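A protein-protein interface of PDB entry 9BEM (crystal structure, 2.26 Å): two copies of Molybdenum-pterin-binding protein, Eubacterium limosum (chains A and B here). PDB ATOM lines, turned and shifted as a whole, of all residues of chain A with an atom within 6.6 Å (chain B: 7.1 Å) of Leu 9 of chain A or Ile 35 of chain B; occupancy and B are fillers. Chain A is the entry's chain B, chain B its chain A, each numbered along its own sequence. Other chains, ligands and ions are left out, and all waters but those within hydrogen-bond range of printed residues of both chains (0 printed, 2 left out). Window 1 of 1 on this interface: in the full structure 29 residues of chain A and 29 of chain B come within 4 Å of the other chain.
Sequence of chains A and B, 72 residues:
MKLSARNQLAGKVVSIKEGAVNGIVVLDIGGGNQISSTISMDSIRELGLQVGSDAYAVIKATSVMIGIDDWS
ND2 of Asn 33 of chain B lies within hydrogen-bond range of O of Ile 29 of chain A (2.8 Å). The backbone NH of Ser 36 of chain B lies within hydrogen-bond range of the side-chain amide oxygen of Asn 7 of chain A, at 2.7 Å. The backbone carbonyl oxygen (O) of Val 64 of chain A sits at hydrogen-bond distance from the side-chain hydroxyl (OG) of Ser 37 of chain B (2.5 Å). The backbone carbonyl oxygen (O) of Gly 67 of chain B lies within hydrogen-bond range of the backbone NH (N) of Tyr 56 of chain A (2.8 Å).
N of Ala 57 of chain B sits at hydrogen-bond distance from O of Leu 9 of chain B (2.9 Å). N of Val 25 of chain B is in hydrogen-bond range of O of Ser 37 of chain B. The backbone carbonyl oxygen (O) of Ile 35 of chain B sits at hydrogen-bond distance from the backbone NH (N) of Leu 27 of chain B (2.8 Å). N of Ile 59 of chain A lies within hydrogen-bond range of O of Asn 7 of chain A (2.9 Å). The backbone NH (N) of Ala 55 of chain A sits at hydrogen-bond distance from the backbone carbonyl oxygen (O) of Gly 11 of chain A, 2.9 Å away. O of Ile 35 of chain A sits at hydrogen-bond distance from N of Leu 27 of chain A, 2.8 Å away.
Leu 9 of chain A touches Ile 35 of chain B, and with the chains exchanged Ile 35 of chain A touches Leu 9 of chain B. Ile 29 of chain B touches its own counterpart, Ile 29 of chain A. Ile 59 of chain A touches its own counterpart, Ile 59 of chain B. 7 positions are printed for both chains.
Arg 6 of chain A touches Ser 36 of chain B. Leu 9 of chain A touches Asn 33 of chain B. Leu 9 of chain A touches Gln 34 of chain B. CD1 of Ile 29 of chain A touches CD1 of Ile 29 of chain B, at 3.9 Å. Gly 67 of chain B touches Ala 55 of chain A (O to CA, 3.2 Å). Ser 36 of chain B touches Val 64 of chain A. CG1 of Val 64 of chain A touches CB of Ala 57 of chain B (3.8 Å). Val 64 of chain A touches Val 58 of chain B. CG1 of Ile 59 of chain B touches CG2 of Val 64 of chain A (3.8 Å). Ile 66 of chain A touches Ser 37 of chain B (CG1 to OG, 3.5 Å).
Leu 9 of chain A touches three residues of chain B. Of the printed residues of chain B, Ile 35 of chain A touches Leu 9 (3.98 Å). Of the printed residues of chain B, Tyr 56 of chain A touches Gly 67 (2.8 Å). Of the printed residues of chain B, Val 64 of chain A touches Ile 35, Ser 36, Ser 37, Ala 57, Val 58 and Ile 59. Asp 28 of chain B touches none of the printed residues of chain A. Printed residues of chain A within 4 Å of Ile 29 of chain B: Ile 29 (3.9 Å). Of the printed residues of chain A, Ser 37 of chain B touches Val 64 (2.5 Å) and Ile 66 (3.5 Å). The nearest residue of chain B that does not touch Leu 9 of chain A is Ile 29 of chain B (5.1 Å). The nearest residue of chain A that does not touch Ile 35 of chain B is Ile 59 of chain A (5.3 Å).
Of the 18 printed residues of chain B, 11 touch a printed residue of chain A. Hydrophobic or aromatic side chains of chain B that line the printed part of chain A: Leu 9, Ile 29, Ile 35, Ala 57 and Ile 59. Of the 16 printed residues of chain A, 10 touch a printed residue of chain B. Printed residues of chain A that touch a printed residue of chain B: Arg 6, Asn 7, Leu 9, Ile 29, Ile 35, Ala 55, Tyr 56, Ile 59, Val 64 and Ile 66. Among the printed residues, 20 pairs touch across the chains.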
ATOM      1  N   ARG A   6       8.325   9.850 -27.433  1.00  0.00           N
ATOM      2  CA  ARG A   6       9.123  10.191 -28.602  1.00  0.00           C
ATOM      3  C   ARG A   6      10.101   9.087 -28.971  1.00  0.00           C
ATOM      4  O   ARG A   6      10.515   9.015 -30.128  1.00  0.00           O
ATOM      5  CB  ARG A   6       9.916  11.478 -28.369  1.00  0.00           C
ATOM      6  CG  ARG A   6       9.092  12.738 -28.147  1.00  0.00           C
ATOM      7  CD  ARG A   6       8.448  13.184 -29.425  1.00  0.00           C
ATOM      8  NE  ARG A   6       7.182  12.487 -29.601  1.00  0.00           N
ATOM      9  CZ  ARG A   6       6.522  12.415 -30.744  1.00  0.00           C
ATOM     10  NH1 ARG A   6       6.986  12.988 -31.843  1.00  0.00           N
ATOM     11  NH2 ARG A   6       5.403  11.692 -30.802  1.00  0.00           N
ATOM     12  N   ASN A   7      10.477   8.212 -28.039  1.00  0.00           N
ATOM     13  CA  ASN A   7      11.480   7.206 -28.354  1.00  0.00           C
ATOM     14  C   ASN A   7      10.854   5.817 -28.345  1.00  0.00           C
ATOM     15  O   ASN A   7      10.422   5.335 -27.291  1.00  0.00           O
ATOM     16  CB  ASN A   7      12.631   7.346 -27.372  1.00  0.00           C
ATOM     17  CG  ASN A   7      13.167   8.752 -27.363  1.00  0.00           C
ATOM     18  OD1 ASN A   7      13.590   9.277 -28.402  1.00  0.00           O
ATOM     19  ND2 ASN A   7      13.072   9.408 -26.213  1.00  0.00           N
ATOM     20  N   GLN A   8      10.817   5.178 -29.521  1.00  0.00           N
ATOM     21  CA  GLN A   8      10.273   3.822 -29.705  1.00  0.00           C
ATOM     22  C   GLN A   8      11.223   3.100 -30.665  1.00  0.00           C
ATOM     23  O   GLN A   8      11.100   3.204 -31.888  1.00  0.00           O
ATOM     24  CB  GLN A   8       8.829   3.829 -30.217  1.00  0.00           C
ATOM     25  CG  GLN A   8       7.933   4.787 -29.394  1.00  0.00           C
ATOM     26  CD  GLN A   8       6.455   4.783 -29.766  1.00  0.00           C
ATOM     27  OE1 GLN A   8       5.957   3.878 -30.442  1.00  0.00           O
ATOM     28  NE2 GLN A   8       5.756   5.849 -29.368  1.00  0.00           N
ATOM     29  N   LEU A   9      12.160   2.355 -30.096  1.00  0.00           N
ATOM     30  CA  LEU A   9      13.335   1.855 -30.798  1.00  0.00           C
ATOM     31  C   LEU A   9      13.215   0.349 -30.943  1.00  0.00           C
ATOM     32  O   LEU A   9      13.280  -0.381 -29.947  1.00  0.00           O
ATOM     33  CB  LEU A   9      14.588   2.238 -30.016  1.00  0.00           C
ATOM     34  CG  LEU A   9      14.718   3.744 -29.880  1.00  0.00           C
ATOM     35  CD1 LEU A   9      15.905   4.036 -29.090  1.00  0.00           C
ATOM     36  CD2 LEU A   9      14.961   4.277 -31.280  1.00  0.00           C
ATOM     37  N   ALA A  10      13.076  -0.106 -32.181  1.00  0.00           N
ATOM     38  CA  ALA A  10      12.924  -1.530 -32.448  1.00  0.00           C
ATOM     39  C   ALA A  10      14.237  -2.260 -32.189  1.00  0.00           C
ATOM     40  O   ALA A  10      15.319  -1.743 -32.483  1.00  0.00           O
ATOM     41  CB  ALA A  10      12.474  -1.755 -33.898  1.00  0.00           C
ATOM     42  N   GLY A  11      14.139  -3.480 -31.668  1.00  0.00           N
ATOM     43  CA  GLY A  11      15.340  -4.243 -31.377  1.00  0.00           C
ATOM     44  C   GLY A  11      15.004  -5.671 -31.012  1.00  0.00           C
ATOM     45  O   GLY A  11      13.840  -6.071 -30.976  1.00  0.00           O
ATOM     46  N   LEU A  27      18.066  -4.905 -25.046  1.00  0.00           N
ATOM     47  CA  LEU A  27      17.625  -4.879 -26.437  1.00  0.00           C
ATOM     48  C   LEU A  27      18.773  -4.432 -27.337  1.00  0.00           C
ATOM     49  O   LEU A  27      19.365  -3.363 -27.111  1.00  0.00           O
ATOM     50  CB  LEU A  27      16.460  -3.907 -26.627  1.00  0.00           C
ATOM     51  CG  LEU A  27      15.036  -4.421 -26.624  1.00  0.00           C
ATOM     52  CD1 LEU A  27      14.084  -3.287 -27.050  1.00  0.00           C
ATOM     53  CD2 LEU A  27      14.909  -5.602 -27.550  1.00  0.00           C
ATOM     54  N   ILE A  29      19.433  -2.697 -30.527  1.00  0.00           N
ATOM     55  CA  ILE A  29      18.637  -1.865 -31.431  1.00  0.00           C
ATOM     56  C   ILE A  29      19.387  -1.532 -32.720  1.00  0.00           C
ATOM     57  O   ILE A  29      18.940  -0.673 -33.485  1.00  0.00           O
ATOM     58  CB  ILE A  29      18.141  -0.580 -30.735  1.00  0.00           C
ATOM     59  CG1 ILE A  29      19.305   0.308 -30.306  1.00  0.00           C
ATOM     60  CG2 ILE A  29      17.257  -0.911 -29.521  1.00  0.00           C
ATOM     61  CD1 ILE A  29      18.894   1.756 -30.141  1.00  0.00           C
ATOM     62  N   ILE A  35      19.988  -1.084 -25.383  1.00  0.00           N
ATOM     63  CA  ILE A  35      19.259  -0.392 -24.334  1.00  0.00           C
ATOM     64  C   ILE A  35      18.861  -1.395 -23.262  1.00  0.00           C
ATOM     65  O   ILE A  35      18.385  -2.493 -23.572  1.00  0.00           O
ATOM     66  CB  ILE A  35      18.018   0.367 -24.860  1.00  0.00           C
ATOM     67  CG1 ILE A  35      18.435   1.546 -25.738  1.00  0.00           C
ATOM     68  CG2 ILE A  35      17.179   0.875 -23.697  1.00  0.00           C
ATOM     69  CD1 ILE A  35      17.485   1.823 -26.822  1.00  0.00           C
ATOM     70  N   ALA A  55      11.129  -6.634 -30.095  1.00  0.00           N
ATOM     71  CA  ALA A  55      10.478  -5.750 -29.138  1.00  0.00           C
ATOM     72  C   ALA A  55      10.880  -4.317 -29.461  1.00  0.00           C
ATOM     73  O   ALA A  55      11.550  -4.057 -30.465  1.00  0.00           O
ATOM     74  CB  ALA A  55      10.824  -6.151 -27.693  1.00  0.00           C
ATOM     75  N   TYR A  56      10.459  -3.388 -28.601  1.00  0.00           N
ATOM     76  CA  TYR A  56      10.770  -1.971 -28.702  1.00  0.00           C
ATOM     77  C   TYR A  56      11.181  -1.426 -27.340  1.00  0.00           C
ATOM     78  O   TYR A  56      10.563  -1.753 -26.321  1.00  0.00           O
ATOM     79  CB  TYR A  56       9.572  -1.140 -29.185  1.00  0.00           C
ATOM     80  CG  TYR A  56       8.980  -1.548 -30.495  1.00  0.00           C
ATOM     81  CD1 TYR A  56       8.111  -2.625 -30.578  1.00  0.00           C
ATOM     82  CD2 TYR A  56       9.255  -0.830 -31.649  1.00  0.00           C
ATOM     83  CE1 TYR A  56       7.560  -2.998 -31.774  1.00  0.00           C
ATOM     84  CE2 TYR A  56       8.704  -1.185 -32.851  1.00  0.00           C
ATOM     85  CZ  TYR A  56       7.856  -2.275 -32.909  1.00  0.00           C
ATOM     86  OH  TYR A  56       7.298  -2.647 -34.101  1.00  0.00           O
ATOM     87  N   ALA A  57      12.202  -0.566 -27.341  1.00  0.00           N
ATOM     88  CA  ALA A  57      12.548   0.267 -26.194  1.00  0.00           C
ATOM     89  C   ALA A  57      11.744   1.556 -26.262  1.00  0.00           C
ATOM     90  O   ALA A  57      11.886   2.326 -27.219  1.00  0.00           O
ATOM     91  CB  ALA A  57      14.043   0.588 -26.182  1.00  0.00           C
ATOM     92  N   VAL A  58      10.930   1.810 -25.244  1.00  0.00           N
ATOM     93  CA  VAL A  58      10.015   2.952 -25.231  1.00  0.00           C
ATOM     94  C   VAL A  58      10.416   3.889 -24.099  1.00  0.00           C
ATOM     95  O   VAL A  58      10.465   3.481 -22.929  1.00  0.00           O
ATOM     96  CB  VAL A  58       8.548   2.514 -25.098  1.00  0.00           C
ATOM     97  CG1 VAL A  58       7.656   3.733 -24.992  1.00  0.00           C
ATOM     98  CG2 VAL A  58       8.140   1.630 -26.313  1.00  0.00           C
ATOM     99  N   ILE A  59      10.748   5.130 -24.458  1.00  0.00           N
ATOM    100  CA  ILE A  59      11.249   6.128 -23.522  1.00  0.00           C
ATOM    101  C   ILE A  59      10.615   7.483 -23.826  1.00  0.00           C
ATOM    102  O   ILE A  59      10.720   8.007 -24.947  1.00  0.00           O
ATOM    103  CB  ILE A  59      12.783   6.247 -23.557  1.00  0.00           C
ATOM    104  CG1 ILE A  59      13.428   4.867 -23.450  1.00  0.00           C
ATOM    105  CG2 ILE A  59      13.272   7.166 -22.431  1.00  0.00           C
ATOM    106  CD1 ILE A  59      14.648   4.731 -24.294  1.00  0.00           C
ATOM    107  N   VAL A  64      15.042  11.501 -20.857  1.00  0.00           N
ATOM    108  CA  VAL A  64      16.355  11.413 -21.491  1.00  0.00           C
ATOM    109  C   VAL A  64      17.157  12.661 -21.161  1.00  0.00           C
ATOM    110  O   VAL A  64      16.708  13.788 -21.406  1.00  0.00           O
ATOM    111  CB  VAL A  64      16.239  11.231 -23.013  1.00  0.00           C
ATOM    112  CG1 VAL A  64      17.620  11.043 -23.630  1.00  0.00           C
ATOM    113  CG2 VAL A  64      15.317  10.052 -23.357  1.00  0.00           C
ATOM    114  N   ILE A  66      21.028  14.655 -21.685  1.00  0.00           N
ATOM    115  CA  ILE A  66      22.121  14.773 -22.641  1.00  0.00           C
ATOM    116  C   ILE A  66      23.428  14.923 -21.879  1.00  0.00           C
ATOM    117  O   ILE A  66      23.500  15.648 -20.880  1.00  0.00           O
ATOM    118  CB  ILE A  66      21.919  15.949 -23.614  1.00  0.00           C
ATOM    119  CG1 ILE A  66      20.658  15.730 -24.460  1.00  0.00           C
ATOM    120  CG2 ILE A  66      23.152  16.128 -24.490  1.00  0.00           C
ATOM    121  CD1 ILE A  66      20.708  14.476 -25.359  1.00  0.00           C
ATOM    122  N   LEU B   9      24.241   6.662 -24.818  1.00  0.00           N
ATOM    123  CA  LEU B   9      24.296   6.321 -26.237  1.00  0.00           C
ATOM    124  C   LEU B   9      24.915   7.478 -27.008  1.00  0.00           C
ATOM    125  O   LEU B   9      24.360   8.578 -27.029  1.00  0.00           O
ATOM    126  CB  LEU B   9      22.896   6.002 -26.769  1.00  0.00           C
ATOM    127  CG  LEU B   9      22.173   4.844 -26.077  1.00  0.00           C
ATOM    128  CD1 LEU B   9      20.810   4.594 -26.673  1.00  0.00           C
ATOM    129  CD2 LEU B   9      23.031   3.588 -26.251  1.00  0.00           C
ATOM    130  N   VAL B  14      21.149  16.523 -34.365  1.00  0.00           N
ATOM    131  CA  VAL B  14      20.605  16.887 -35.675  1.00  0.00           C
ATOM    132  C   VAL B  14      19.629  18.061 -35.574  1.00  0.00           C
ATOM    133  O   VAL B  14      19.447  18.799 -36.549  1.00  0.00           O
ATOM    134  CB  VAL B  14      19.947  15.678 -36.374  1.00  0.00           C
ATOM    135  CG1 VAL B  14      21.011  14.635 -36.684  1.00  0.00           C
ATOM    136  CG2 VAL B  14      18.860  15.071 -35.530  1.00  0.00           C
ATOM    137  N   ILE B  24      13.987  20.594 -26.843  1.00  0.00           N
ATOM    138  CA  ILE B  24      14.035  19.194 -27.272  1.00  0.00           C
ATOM    139  C   ILE B  24      15.234  18.995 -28.197  1.00  0.00           C
ATOM    140  O   ILE B  24      15.291  19.577 -29.286  1.00  0.00           O
ATOM    141  CB  ILE B  24      12.729  18.773 -27.956  1.00  0.00           C
ATOM    142  CG1 ILE B  24      11.549  18.997 -27.011  1.00  0.00           C
ATOM    143  CG2 ILE B  24      12.778  17.315 -28.397  1.00  0.00           C
ATOM    144  CD1 ILE B  24      10.229  18.606 -27.630  1.00  0.00           C
ATOM    145  N   VAL B  25      16.181  18.168 -27.760  1.00  0.00           N
ATOM    146  CA  VAL B  25      17.388  17.834 -28.512  1.00  0.00           C
ATOM    147  C   VAL B  25      17.186  16.484 -29.176  1.00  0.00           C
ATOM    148  O   VAL B  25      16.839  15.508 -28.509  1.00  0.00           O
ATOM    149  CB  VAL B  25      18.621  17.790 -27.596  1.00  0.00           C
ATOM    150  CG1 VAL B  25      19.840  17.352 -28.392  1.00  0.00           C
ATOM    151  CG2 VAL B  25      18.849  19.149 -26.948  1.00  0.00           C
ATOM    152  N   VAL B  26      17.407  16.413 -30.482  1.00  0.00           N
ATOM    153  CA  VAL B  26      17.329  15.154 -31.212  1.00  0.00           C
ATOM    154  C   VAL B  26      18.739  14.726 -31.573  1.00  0.00           C
ATOM    155  O   VAL B  26      19.497  15.496 -32.179  1.00  0.00           O
ATOM    156  CB  VAL B  26      16.442  15.250 -32.460  1.00  0.00           C
ATOM    157  CG1 VAL B  26      16.416  13.911 -33.166  1.00  0.00           C
ATOM    158  CG2 VAL B  26      15.016  15.631 -32.060  1.00  0.00           C
ATOM    159  N   LEU B  27      19.072  13.491 -31.207  1.00  0.00           N
ATOM    160  CA  LEU B  27      20.390  12.905 -31.346  1.00  0.00           C
ATOM    161  C   LEU B  27      20.300  11.750 -32.333  1.00  0.00           C
ATOM    162  O   LEU B  27      19.475  10.853 -32.160  1.00  0.00           O
ATOM    163  CB  LEU B  27      20.861  12.388 -29.978  1.00  0.00           C
ATOM    164  CG  LEU B  27      22.300  12.542 -29.540  1.00  0.00           C
ATOM    165  CD1 LEU B  27      22.566  14.023 -29.310  1.00  0.00           C
ATOM    166  CD2 LEU B  27      22.575  11.718 -28.285  1.00  0.00           C
ATOM    167  N   ASP B  28      21.130  11.770 -33.366  1.00  0.00           N
ATOM    168  CA  ASP B  28      21.291  10.633 -34.263  1.00  0.00           C
ATOM    169  C   ASP B  28      22.328   9.699 -33.644  1.00  0.00           C
ATOM    170  O   ASP B  28      23.505  10.064 -33.536  1.00  0.00           O
ATOM    171  CB  ASP B  28      21.709  11.118 -35.652  1.00  0.00           C
ATOM    172  CG  ASP B  28      21.732  10.015 -36.694  1.00  0.00           C
ATOM    173  OD1 ASP B  28      22.125   8.874 -36.390  1.00  0.00           O
ATOM    174  OD2 ASP B  28      21.310  10.289 -37.840  1.00  0.00           O
ATOM    175  N   ILE B  29      21.902   8.504 -33.226  1.00  0.00           N
ATOM    176  CA  ILE B  29      22.825   7.581 -32.576  1.00  0.00           C
ATOM    177  C   ILE B  29      23.263   6.457 -33.509  1.00  0.00           C
ATOM    178  O   ILE B  29      23.855   5.477 -33.055  1.00  0.00           O
ATOM    179  CB  ILE B  29      22.241   7.029 -31.265  1.00  0.00           C
ATOM    180  CG1 ILE B  29      20.984   6.204 -31.526  1.00  0.00           C
ATOM    181  CG2 ILE B  29      21.940   8.172 -30.284  1.00  0.00           C
ATOM    182  CD1 ILE B  29      20.684   5.225 -30.396  1.00  0.00           C
ATOM    183  N   GLY B  32      20.184   4.158 -37.986  1.00  0.00           N
ATOM    184  CA  GLY B  32      18.851   4.640 -38.275  1.00  0.00           C
ATOM    185  C   GLY B  32      18.035   5.059 -37.065  1.00  0.00           C
ATOM    186  O   GLY B  32      16.852   5.375 -37.216  1.00  0.00           O
ATOM    187  N   ASN B  33      18.627   5.099 -35.873  1.00  0.00           N
ATOM    188  CA  ASN B  33      17.892   5.446 -34.663  1.00  0.00           C
ATOM    189  C   ASN B  33      18.181   6.878 -34.231  1.00  0.00           C
ATOM    190  O   ASN B  33      19.327   7.351 -34.290  1.00  0.00           O
ATOM    191  CB  ASN B  33      18.249   4.493 -33.526  1.00  0.00           C
ATOM    192  CG  ASN B  33      17.747   3.089 -33.774  1.00  0.00           C
ATOM    193  OD1 ASN B  33      16.599   2.880 -34.182  1.00  0.00           O
ATOM    194  ND2 ASN B  33      18.612   2.112 -33.533  1.00  0.00           N
ATOM    195  N   GLN B  34      17.140   7.556 -33.760  1.00  0.00           N
ATOM    196  CA  GLN B  34      17.303   8.872 -33.171  1.00  0.00           C
ATOM    197  C   GLN B  34      16.662   8.874 -31.791  1.00  0.00           C
ATOM    198  O   GLN B  34      15.697   8.155 -31.543  1.00  0.00           O
ATOM    199  CB  GLN B  34      16.711   9.957 -34.074  1.00  0.00           C
ATOM    200  CG  GLN B  34      17.366   9.953 -35.452  1.00  0.00           C
ATOM    201  CD  GLN B  34      16.935  11.119 -36.305  1.00  0.00           C
ATOM    202  OE1 GLN B  34      15.965  11.803 -35.987  1.00  0.00           O
ATOM    203  NE2 GLN B  34      17.630  11.327 -37.422  1.00  0.00           N
ATOM    204  N   ILE B  35      17.232   9.655 -30.880  1.00  0.00           N
ATOM    205  CA  ILE B  35      16.714   9.801 -29.527  1.00  0.00           C
ATOM    206  C   ILE B  35      16.337  11.261 -29.324  1.00  0.00           C
ATOM    207  O   ILE B  35      17.152  12.153 -29.587  1.00  0.00           O
ATOM    208  CB  ILE B  35      17.760   9.408 -28.472  1.00  0.00           C
ATOM    209  CG1 ILE B  35      18.248   7.979 -28.668  1.00  0.00           C
ATOM    210  CG2 ILE B  35      17.123   9.490 -27.075  1.00  0.00           C
ATOM    211  CD1 ILE B  35      17.249   6.969 -28.380  1.00  0.00           C
ATOM    212  N   SER B  36      15.133  11.506 -28.819  1.00  0.00           N
ATOM    213  CA  SER B  36      14.712  12.848 -28.437  1.00  0.00           C
ATOM    214  C   SER B  36      14.823  12.987 -26.926  1.00  0.00           C
ATOM    215  O   SER B  36      14.437  12.080 -26.182  1.00  0.00           O
ATOM    216  CB  SER B  36      13.273  13.148 -28.868  1.00  0.00           C
ATOM    217  OG  SER B  36      13.127  13.145 -30.277  1.00  0.00           O
ATOM    218  N   SER B  37      15.345  14.137 -26.488  1.00  0.00           N
ATOM    219  CA  SER B  37      15.588  14.451 -25.084  1.00  0.00           C
ATOM    220  C   SER B  37      14.989  15.822 -24.783  1.00  0.00           C
ATOM    221  O   SER B  37      15.311  16.803 -25.467  1.00  0.00           O
ATOM    222  CB  SER B  37      17.081  14.459 -24.761  1.00  0.00           C
ATOM    223  OG  SER B  37      17.322  15.043 -23.494  1.00  0.00           O
ATOM    224  N   ALA B  57      22.900  10.356 -25.315  1.00  0.00           N
ATOM    225  CA  ALA B  57      21.585  10.241 -24.707  1.00  0.00           C
ATOM    226  C   ALA B  57      21.730   9.365 -23.471  1.00  0.00           C
ATOM    227  O   ALA B  57      22.164   8.208 -23.568  1.00  0.00           O
ATOM    228  CB  ALA B  57      20.566   9.653 -25.681  1.00  0.00           C
ATOM    229  N   VAL B  58      21.374   9.910 -22.316  1.00  0.00           N
ATOM    230  CA  VAL B  58      21.604   9.253 -21.040  1.00  0.00           C
ATOM    231  C   VAL B  58      20.248   8.926 -20.434  1.00  0.00           C
ATOM    232  O   VAL B  58      19.448   9.829 -20.149  1.00  0.00           O
ATOM    233  CB  VAL B  58      22.444  10.139 -20.111  1.00  0.00           C
ATOM    234  CG1 VAL B  58      22.592   9.509 -18.765  1.00  0.00           C
ATOM    235  CG2 VAL B  58      23.811  10.426 -20.757  1.00  0.00           C
ATOM    236  N   ILE B  59      19.995   7.633 -20.227  1.00  0.00           N
ATOM    237  CA  ILE B  59      18.692   7.152 -19.780  1.00  0.00           C
ATOM    238  C   ILE B  59      18.871   6.108 -18.689  1.00  0.00           C
ATOM    239  O   ILE B  59      19.550   5.080 -18.875  1.00  0.00           O
ATOM    240  CB  ILE B  59      17.862   6.549 -20.922  1.00  0.00           C
ATOM    241  CG1 ILE B  59      17.867   7.490 -22.114  1.00  0.00           C
ATOM    242  CG2 ILE B  59      16.463   6.321 -20.430  1.00  0.00           C
ATOM    243  CD1 ILE B  59      17.905   6.778 -23.428  1.00  0.00           C
ATOM    244  N   GLY B  67       7.944  -2.592 -25.511  1.00  0.00           N
ATOM    245  CA  GLY B  67       6.758  -2.879 -26.289  1.00  0.00           C
ATOM    246  C   GLY B  67       6.918  -4.031 -27.263  1.00  0.00           C
ATOM    247  O   GLY B  67       8.041  -4.397 -27.627  1.00  0.00           O
